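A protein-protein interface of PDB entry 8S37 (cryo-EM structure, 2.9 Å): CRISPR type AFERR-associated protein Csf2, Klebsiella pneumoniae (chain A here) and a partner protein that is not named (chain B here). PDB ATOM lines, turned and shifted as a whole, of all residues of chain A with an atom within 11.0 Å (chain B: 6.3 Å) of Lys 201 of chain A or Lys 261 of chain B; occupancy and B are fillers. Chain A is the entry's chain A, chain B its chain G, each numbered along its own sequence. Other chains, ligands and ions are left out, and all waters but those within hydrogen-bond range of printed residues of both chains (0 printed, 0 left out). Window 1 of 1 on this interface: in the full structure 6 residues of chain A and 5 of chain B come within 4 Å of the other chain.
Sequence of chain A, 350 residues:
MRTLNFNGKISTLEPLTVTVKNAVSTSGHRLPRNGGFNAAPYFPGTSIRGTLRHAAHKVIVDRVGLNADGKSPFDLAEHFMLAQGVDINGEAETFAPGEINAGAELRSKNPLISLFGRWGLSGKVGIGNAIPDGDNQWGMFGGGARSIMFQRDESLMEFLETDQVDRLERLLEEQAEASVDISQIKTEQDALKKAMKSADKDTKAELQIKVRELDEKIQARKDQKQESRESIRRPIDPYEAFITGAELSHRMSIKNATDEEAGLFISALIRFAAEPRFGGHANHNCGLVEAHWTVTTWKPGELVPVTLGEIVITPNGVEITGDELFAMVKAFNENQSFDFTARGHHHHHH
Lys 197 of chain A touches none of the printed residues of chain B.
Of the printed residues of chain B, Ala 199 of chain A touches Lys 207.
Printed residues of chain B within 4 Å of Asp 200 of chain A: Lys 207 (3.6 Å).
Of chain B, only Lys 261 (3.8 Å) and Lys 262 (3.8 Å) come within 4 Å of Lys 201 of chain A.
Thr 203 of chain A touches none of the printed residues of chain B.
Printed residues of chain A within 4 Å of Lys 207 of chain B: Ala 199 (3.1 Å) and Asp 200 (3.6 Å).
No residue of chain A comes within 4 Å of Leu 260 of chain B.
Lys 261 of chain B touches just one residue of chain A: Lys 201 (3.8 Å).
Of chain A, only Lys 201 comes within 4 Å of Lys 262 of chain B.
Val 263 of chain B touches none of the printed residues of chain A.
The nearest residue of chain B that does not touch Lys 201 of chain A is Val 263 of chain B (4.3 Å).
Of the 12 printed residues of chain B, 3 touch a printed residue of chain A.
Printed residues of chain B that touch a printed residue of chain A: Lys 207, Lys 261 and Lys 262.
Lys 261 of chain B touches Lys 201 of chain A.
NZ of Lys 201 of chain A touches O of Lys 262 of chain B, 3.8 Å away.
O of Ala 199 of chain A is in hydrogen-bond range of NZ of Lys 207 of chain B (3.1 Å).
The side-chain carboxylate (OD1) of Asp 200 of chain A is in salt-bridge range of the side-chain amino group (NZ) of Lys 207 of chain B, 3.8 Å away.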
ATOM      1  N   ALA A 195      -1.075 -14.787  12.528  1.00  0.00           N
ATOM      2  CA  ALA A 195      -0.756 -15.724  11.454  1.00  0.00           C
ATOM      3  C   ALA A 195       0.660 -15.520  10.931  1.00  0.00           C
ATOM      4  O   ALA A 195       1.267 -16.462  10.408  1.00  0.00           O
ATOM      5  CB  ALA A 195      -1.764 -15.579  10.316  1.00  0.00           C
ATOM      6  N   MET A 196       1.192 -14.300  11.049  1.00  0.00           N
ATOM      7  CA  MET A 196       2.577 -14.042  10.658  1.00  0.00           C
ATOM      8  C   MET A 196       3.553 -14.971  11.369  1.00  0.00           C
ATOM      9  O   MET A 196       4.627 -15.268  10.834  1.00  0.00           O
ATOM     10  CB  MET A 196       2.964 -12.585  10.936  1.00  0.00           C
ATOM     11  CG  MET A 196       2.228 -11.528  10.109  1.00  0.00           C
ATOM     12  SD  MET A 196       2.076 -11.882   8.346  1.00  0.00           S
ATOM     13  CE  MET A 196       2.976 -10.504   7.639  1.00  0.00           C
ATOM     14  N   LYS A 197       3.213 -15.431  12.574  1.00  0.00           N
ATOM     15  CA  LYS A 197       4.159 -16.220  13.354  1.00  0.00           C
ATOM     16  C   LYS A 197       4.311 -17.636  12.812  1.00  0.00           C
ATOM     17  O   LYS A 197       5.337 -18.275  13.070  1.00  0.00           O
ATOM     18  CB  LYS A 197       3.720 -16.275  14.818  1.00  0.00           C
ATOM     19  CG  LYS A 197       3.327 -14.926  15.421  1.00  0.00           C
ATOM     20  CD  LYS A 197       4.385 -13.838  15.224  1.00  0.00           C
ATOM     21  CE  LYS A 197       5.734 -14.218  15.824  1.00  0.00           C
ATOM     22  NZ  LYS A 197       5.635 -14.551  17.273  1.00  0.00           N
ATOM     23  N   SER A 198       3.321 -18.139  12.076  1.00  0.00           N
ATOM     24  CA  SER A 198       3.437 -19.400  11.356  1.00  0.00           C
ATOM     25  C   SER A 198       3.907 -19.205   9.917  1.00  0.00           C
ATOM     26  O   SER A 198       3.715 -20.103   9.087  1.00  0.00           O
ATOM     27  CB  SER A 198       2.097 -20.139  11.373  1.00  0.00           C
ATOM     28  OG  SER A 198       1.094 -19.386  10.715  1.00  0.00           O
ATOM     29  N   ALA A 199       4.472 -18.036   9.605  1.00  0.00           N
ATOM     30  CA  ALA A 199       5.031 -17.719   8.295  1.00  0.00           C
ATOM     31  C   ALA A 199       5.815 -18.876   7.691  1.00  0.00           C
ATOM     32  O   ALA A 199       6.690 -19.458   8.337  1.00  0.00           O
ATOM     33  CB  ALA A 199       5.937 -16.491   8.404  1.00  0.00           C
ATOM     34  N   ASP A 200       5.485 -19.203   6.442  1.00  0.00           N
ATOM     35  CA  ASP A 200       6.293 -20.077   5.604  1.00  0.00           C
ATOM     36  C   ASP A 200       6.945 -19.317   4.454  1.00  0.00           C
ATOM     37  O   ASP A 200       7.676 -19.920   3.661  1.00  0.00           O
ATOM     38  CB  ASP A 200       5.432 -21.222   5.055  1.00  0.00           C
ATOM     39  CG  ASP A 200       6.260 -22.369   4.495  1.00  0.00           C
ATOM     40  OD1 ASP A 200       7.498 -22.360   4.662  1.00  0.00           O
ATOM     41  OD2 ASP A 200       5.668 -23.283   3.884  1.00  0.00           O
ATOM     42  N   LYS A 201       6.695 -18.013   4.345  1.00  0.00           N
ATOM     43  CA  LYS A 201       7.228 -17.077   3.359  1.00  0.00           C
ATOM     44  C   LYS A 201       6.575 -17.247   1.990  1.00  0.00           C
ATOM     45  O   LYS A 201       6.869 -16.453   1.087  1.00  0.00           O
ATOM     46  CB  LYS A 201       8.754 -17.197   3.206  1.00  0.00           C
ATOM     47  CG  LYS A 201       9.415 -16.011   2.516  1.00  0.00           C
ATOM     48  CD  LYS A 201      10.926 -16.045   2.675  1.00  0.00           C
ATOM     49  CE  LYS A 201      11.598 -14.947   1.863  1.00  0.00           C
ATOM     50  NZ  LYS A 201      11.132 -13.587   2.252  1.00  0.00           N
ATOM     51  N   ASP A 202       5.686 -18.225   1.803  1.00  0.00           N
ATOM     52  CA  ASP A 202       4.839 -18.225   0.617  1.00  0.00           C
ATOM     53  C   ASP A 202       3.701 -17.223   0.761  1.00  0.00           C
ATOM     54  O   ASP A 202       3.342 -16.538  -0.204  1.00  0.00           O
ATOM     55  CB  ASP A 202       4.286 -19.629   0.370  1.00  0.00           C
ATOM     56  CG  ASP A 202       5.380 -20.664   0.204  1.00  0.00           C
ATOM     57  OD1 ASP A 202       6.467 -20.306  -0.296  1.00  0.00           O
ATOM     58  OD2 ASP A 202       5.154 -21.835   0.575  1.00  0.00           O
ATOM     59  N   THR A 203       3.129 -17.130   1.962  1.00  0.00           N
ATOM     60  CA  THR A 203       2.049 -16.188   2.225  1.00  0.00           C
ATOM     61  C   THR A 203       2.565 -14.792   2.545  1.00  0.00           C
ATOM     62  O   THR A 203       1.860 -13.806   2.299  1.00  0.00           O
ATOM     63  CB  THR A 203       1.184 -16.693   3.382  1.00  0.00           C
ATOM     64  OG1 THR A 203       1.979 -16.789   4.569  1.00  0.00           O
ATOM     65  CG2 THR A 203       0.600 -18.061   3.055  1.00  0.00           C
ATOM     66  N   LYS A 204       3.784 -14.685   3.083  1.00  0.00           N
ATOM     67  CA  LYS A 204       4.237 -13.412   3.633  1.00  0.00           C
ATOM     68  C   LYS A 204       4.366 -12.341   2.564  1.00  0.00           C
ATOM     69  O   LYS A 204       4.178 -11.155   2.854  1.00  0.00           O
ATOM     70  CB  LYS A 204       5.575 -13.598   4.347  1.00  0.00           C
ATOM     71  CG  LYS A 204       5.465 -14.335   5.667  1.00  0.00           C
ATOM     72  CD  LYS A 204       5.010 -13.399   6.777  1.00  0.00           C
ATOM     73  CE  LYS A 204       6.178 -12.633   7.380  1.00  0.00           C
ATOM     74  NZ  LYS A 204       7.103 -13.512   8.153  1.00  0.00           N
ATOM     75  N   ALA A 205       4.693 -12.725   1.328  1.00  0.00           N
ATOM     76  CA  ALA A 205       4.714 -11.745   0.250  1.00  0.00           C
ATOM     77  C   ALA A 205       3.346 -11.114   0.020  1.00  0.00           C
ATOM     78  O   ALA A 205       3.268 -10.015  -0.539  1.00  0.00           O
ATOM     79  CB  ALA A 205       5.206 -12.399  -1.041  1.00  0.00           C
ATOM     80  N   GLU A 206       2.272 -11.780   0.447  1.00  0.00           N
ATOM     81  CA  GLU A 206       0.910 -11.270   0.361  1.00  0.00           C
ATOM     82  C   GLU A 206       0.394 -10.720   1.683  1.00  0.00           C
ATOM     83  O   GLU A 206      -0.406  -9.781   1.687  1.00  0.00           O
ATOM     84  CB  GLU A 206      -0.031 -12.375  -0.136  1.00  0.00           C
ATOM     85  CG  GLU A 206      -1.501 -11.961  -0.263  1.00  0.00           C
ATOM     86  CD  GLU A 206      -2.322 -12.211   0.998  1.00  0.00           C
ATOM     87  OE1 GLU A 206      -1.765 -12.696   2.005  1.00  0.00           O
ATOM     88  OE2 GLU A 206      -3.536 -11.914   0.979  1.00  0.00           O
ATOM     89  N   LEU A 207       0.789 -11.323   2.807  1.00  0.00           N
ATOM     90  CA  LEU A 207       0.166 -10.981   4.080  1.00  0.00           C
ATOM     91  C   LEU A 207       0.448  -9.540   4.487  1.00  0.00           C
ATOM     92  O   LEU A 207      -0.447  -8.851   4.986  1.00  0.00           O
ATOM     93  CB  LEU A 207       0.636 -11.945   5.167  1.00  0.00           C
ATOM     94  CG  LEU A 207       0.094 -13.372   5.054  1.00  0.00           C
ATOM     95  CD1 LEU A 207       0.836 -14.291   6.003  1.00  0.00           C
ATOM     96  CD2 LEU A 207      -1.405 -13.413   5.330  1.00  0.00           C
ATOM     97  N   GLN A 208       1.687  -9.072   4.325  1.00  0.00           N
ATOM     98  CA  GLN A 208       1.992  -7.707   4.746  1.00  0.00           C
ATOM     99  C   GLN A 208       1.231  -6.684   3.908  1.00  0.00           C
ATOM    100  O   GLN A 208       0.724  -5.688   4.442  1.00  0.00           O
ATOM    101  CB  GLN A 208       3.505  -7.460   4.686  1.00  0.00           C
ATOM    102  CG  GLN A 208       4.105  -7.143   3.309  1.00  0.00           C
ATOM    103  CD  GLN A 208       3.909  -8.248   2.291  1.00  0.00           C
ATOM    104  OE1 GLN A 208       2.885  -8.934   2.285  1.00  0.00           O
ATOM    105  NE2 GLN A 208       4.887  -8.419   1.414  1.00  0.00           N
ATOM    106  N   LYS B 207      13.494 -24.824  10.348  1.00  0.00           N
ATOM    107  CA  LYS B 207      12.774 -23.566  10.175  1.00  0.00           C
ATOM    108  C   LYS B 207      12.325 -23.014  11.519  1.00  0.00           C
ATOM    109  O   LYS B 207      12.402 -21.804  11.761  1.00  0.00           O
ATOM    110  CB  LYS B 207      11.577 -23.776   9.245  1.00  0.00           C
ATOM    111  CG  LYS B 207      10.656 -22.567   9.081  1.00  0.00           C
ATOM    112  CD  LYS B 207      11.405 -21.327   8.609  1.00  0.00           C
ATOM    113  CE  LYS B 207      10.461 -20.157   8.379  1.00  0.00           C
ATOM    114  NZ  LYS B 207       9.463 -20.428   7.309  1.00  0.00           N
ATOM    115  N   MET B 210      15.342 -21.747  13.123  1.00  0.00           N
ATOM    116  CA  MET B 210      15.756 -20.495  12.509  1.00  0.00           C
ATOM    117  C   MET B 210      14.910 -19.334  13.014  1.00  0.00           C
ATOM    118  O   MET B 210      15.442 -18.264  13.332  1.00  0.00           O
ATOM    119  CB  MET B 210      15.664 -20.611  10.988  1.00  0.00           C
ATOM    120  CG  MET B 210      15.632 -19.287  10.234  1.00  0.00           C
ATOM    121  SD  MET B 210      15.829 -19.518   8.457  1.00  0.00           S
ATOM    122  CE  MET B 210      15.388 -17.891   7.853  1.00  0.00           C
ATOM    123  N   ILE B 214      16.334 -16.162  15.138  1.00  0.00           N
ATOM    124  CA  ILE B 214      16.166 -14.800  14.639  1.00  0.00           C
ATOM    125  C   ILE B 214      15.452 -13.945  15.676  1.00  0.00           C
ATOM    126  O   ILE B 214      15.869 -12.821  15.973  1.00  0.00           O
ATOM    127  CB  ILE B 214      15.412 -14.811  13.298  1.00  0.00           C
ATOM    128  CG1 ILE B 214      16.307 -15.391  12.199  1.00  0.00           C
ATOM    129  CG2 ILE B 214      14.946 -13.406  12.931  1.00  0.00           C
ATOM    130  CD1 ILE B 214      15.553 -15.852  10.966  1.00  0.00           C
ATOM    131  N   THR B 218      17.009 -10.766  17.667  1.00  0.00           N
ATOM    132  CA  THR B 218      16.374  -9.466  17.489  1.00  0.00           C
ATOM    133  C   THR B 218      15.945  -8.877  18.827  1.00  0.00           C
ATOM    134  O   THR B 218      16.173  -7.693  19.098  1.00  0.00           O
ATOM    135  CB  THR B 218      15.169  -9.596  16.557  1.00  0.00           C
ATOM    136  OG1 THR B 218      15.561 -10.269  15.354  1.00  0.00           O
ATOM    137  CG2 THR B 218      14.612  -8.227  16.207  1.00  0.00           C
ATOM    138  N   ILE B 256      22.264  -7.985   9.786  1.00  0.00           N
ATOM    139  CA  ILE B 256      22.441  -9.318   9.225  1.00  0.00           C
ATOM    140  C   ILE B 256      21.164 -10.133   9.373  1.00  0.00           C
ATOM    141  O   ILE B 256      20.857 -10.977   8.523  1.00  0.00           O
ATOM    142  CB  ILE B 256      23.640 -10.011   9.896  1.00  0.00           C
ATOM    143  CG1 ILE B 256      24.944  -9.310   9.503  1.00  0.00           C
ATOM    144  CG2 ILE B 256      23.689 -11.478   9.512  1.00  0.00           C
ATOM    145  CD1 ILE B 256      26.089  -9.568  10.454  1.00  0.00           C
ATOM    146  N   LEU B 257      20.384  -9.886  10.425  1.00  0.00           N
ATOM    147  CA  LEU B 257      19.086 -10.538  10.547  1.00  0.00           C
ATOM    148  C   LEU B 257      18.133 -10.058   9.464  1.00  0.00           C
ATOM    149  O   LEU B 257      17.395 -10.860   8.879  1.00  0.00           O
ATOM    150  CB  LEU B 257      18.492 -10.279  11.927  1.00  0.00           C
ATOM    151  CG  LEU B 257      19.129 -11.007  13.108  1.00  0.00           C
ATOM    152  CD1 LEU B 257      18.566 -10.432  14.392  1.00  0.00           C
ATOM    153  CD2 LEU B 257      18.895 -12.508  13.033  1.00  0.00           C
ATOM    154  N   HIS B 258      18.093  -8.745   9.227  1.00  0.00           N
ATOM    155  CA  HIS B 258      17.320  -8.207   8.114  1.00  0.00           C
ATOM    156  C   HIS B 258      17.735  -8.866   6.807  1.00  0.00           C
ATOM    157  O   HIS B 258      16.889  -9.225   5.979  1.00  0.00           O
ATOM    158  CB  HIS B 258      17.509  -6.693   8.042  1.00  0.00           C
ATOM    159  CG  HIS B 258      16.669  -6.026   7.001  1.00  0.00           C
ATOM    160  ND1 HIS B 258      17.122  -4.961   6.251  1.00  0.00           N
ATOM    161  CD2 HIS B 258      15.402  -6.262   6.589  1.00  0.00           C
ATOM    162  CE1 HIS B 258      16.172  -4.575   5.419  1.00  0.00           C
ATOM    163  NE2 HIS B 258      15.117  -5.347   5.604  1.00  0.00           N
ATOM    164  N   LEU B 259      19.039  -9.076   6.629  1.00  0.00           N
ATOM    165  CA  LEU B 259      19.530  -9.673   5.393  1.00  0.00           C
ATOM    166  C   LEU B 259      19.098 -11.128   5.289  1.00  0.00           C
ATOM    167  O   LEU B 259      18.742 -11.599   4.204  1.00  0.00           O
ATOM    168  CB  LEU B 259      21.057  -9.552   5.345  1.00  0.00           C
ATOM    169  CG  LEU B 259      21.896 -10.176   4.217  1.00  0.00           C
ATOM    170  CD1 LEU B 259      22.016 -11.698   4.313  1.00  0.00           C
ATOM    171  CD2 LEU B 259      21.362  -9.778   2.857  1.00  0.00           C
ATOM    172  N   LEU B 260      19.118 -11.855   6.404  1.00  0.00           N
ATOM    173  CA  LEU B 260      18.693 -13.248   6.376  1.00  0.00           C
ATOM    174  C   LEU B 260      17.203 -13.361   6.086  1.00  0.00           C
ATOM    175  O   LEU B 260      16.789 -14.132   5.211  1.00  0.00           O
ATOM    176  CB  LEU B 260      19.028 -13.929   7.702  1.00  0.00           C
ATOM    177  CG  LEU B 260      20.491 -14.276   7.971  1.00  0.00           C
ATOM    178  CD1 LEU B 260      20.630 -14.803   9.391  1.00  0.00           C
ATOM    179  CD2 LEU B 260      21.018 -15.292   6.964  1.00  0.00           C
ATOM    180  N   LYS B 261      16.377 -12.604   6.806  1.00  0.00           N
ATOM    181  CA  LYS B 261      14.937 -12.711   6.615  1.00  0.00           C
ATOM    182  C   LYS B 261      14.446 -11.997   5.363  1.00  0.00           C
ATOM    183  O   LYS B 261      13.252 -12.083   5.057  1.00  0.00           O
ATOM    184  CB  LYS B 261      14.196 -12.167   7.842  1.00  0.00           C
ATOM    185  CG  LYS B 261      14.239 -10.647   8.013  1.00  0.00           C
ATOM    186  CD  LYS B 261      13.485 -10.188   9.256  1.00  0.00           C
ATOM    187  CE  LYS B 261      14.173 -10.614  10.544  1.00  0.00           C
ATOM    188  NZ  LYS B 261      13.516 -10.021  11.742  1.00  0.00           N
ATOM    189  N   LYS B 262      15.322 -11.304   4.634  1.00  0.00           N
ATOM    190  CA  LYS B 262      14.963 -10.799   3.316  1.00  0.00           C
ATOM    191  C   LYS B 262      15.181 -11.841   2.228  1.00  0.00           C
ATOM    192  O   LYS B 262      14.411 -11.898   1.264  1.00  0.00           O
ATOM    193  CB  LYS B 262      15.755  -9.527   3.002  1.00  0.00           C
ATOM    194  CG  LYS B 262      15.184  -8.276   3.660  1.00  0.00           C
ATOM    195  CD  LYS B 262      13.890  -7.822   2.999  1.00  0.00           C
ATOM    196  CE  LYS B 262      12.828  -7.477   4.030  1.00  0.00           C
ATOM    197  NZ  LYS B 262      11.539  -7.086   3.398  1.00  0.00           N
ATOM    198  N   VAL B 263      16.215 -12.667   2.367  1.00  0.00           N
ATOM    199  CA  VAL B 263      16.512 -13.705   1.388  1.00  0.00           C
ATOM    200  C   VAL B 263      15.889 -15.024   1.827  1.00  0.00           C
ATOM    201  O   VAL B 263      15.760 -15.293   3.020  1.00  0.00           O
ATOM    202  CB  VAL B 263      18.031 -13.860   1.183  1.00  0.00           C
ATOM    203  CG1 VAL B 263      18.660 -12.509   0.900  1.00  0.00           C
ATOM    204  CG2 VAL B 263      18.681 -14.516   2.395  1.00  0.00           C
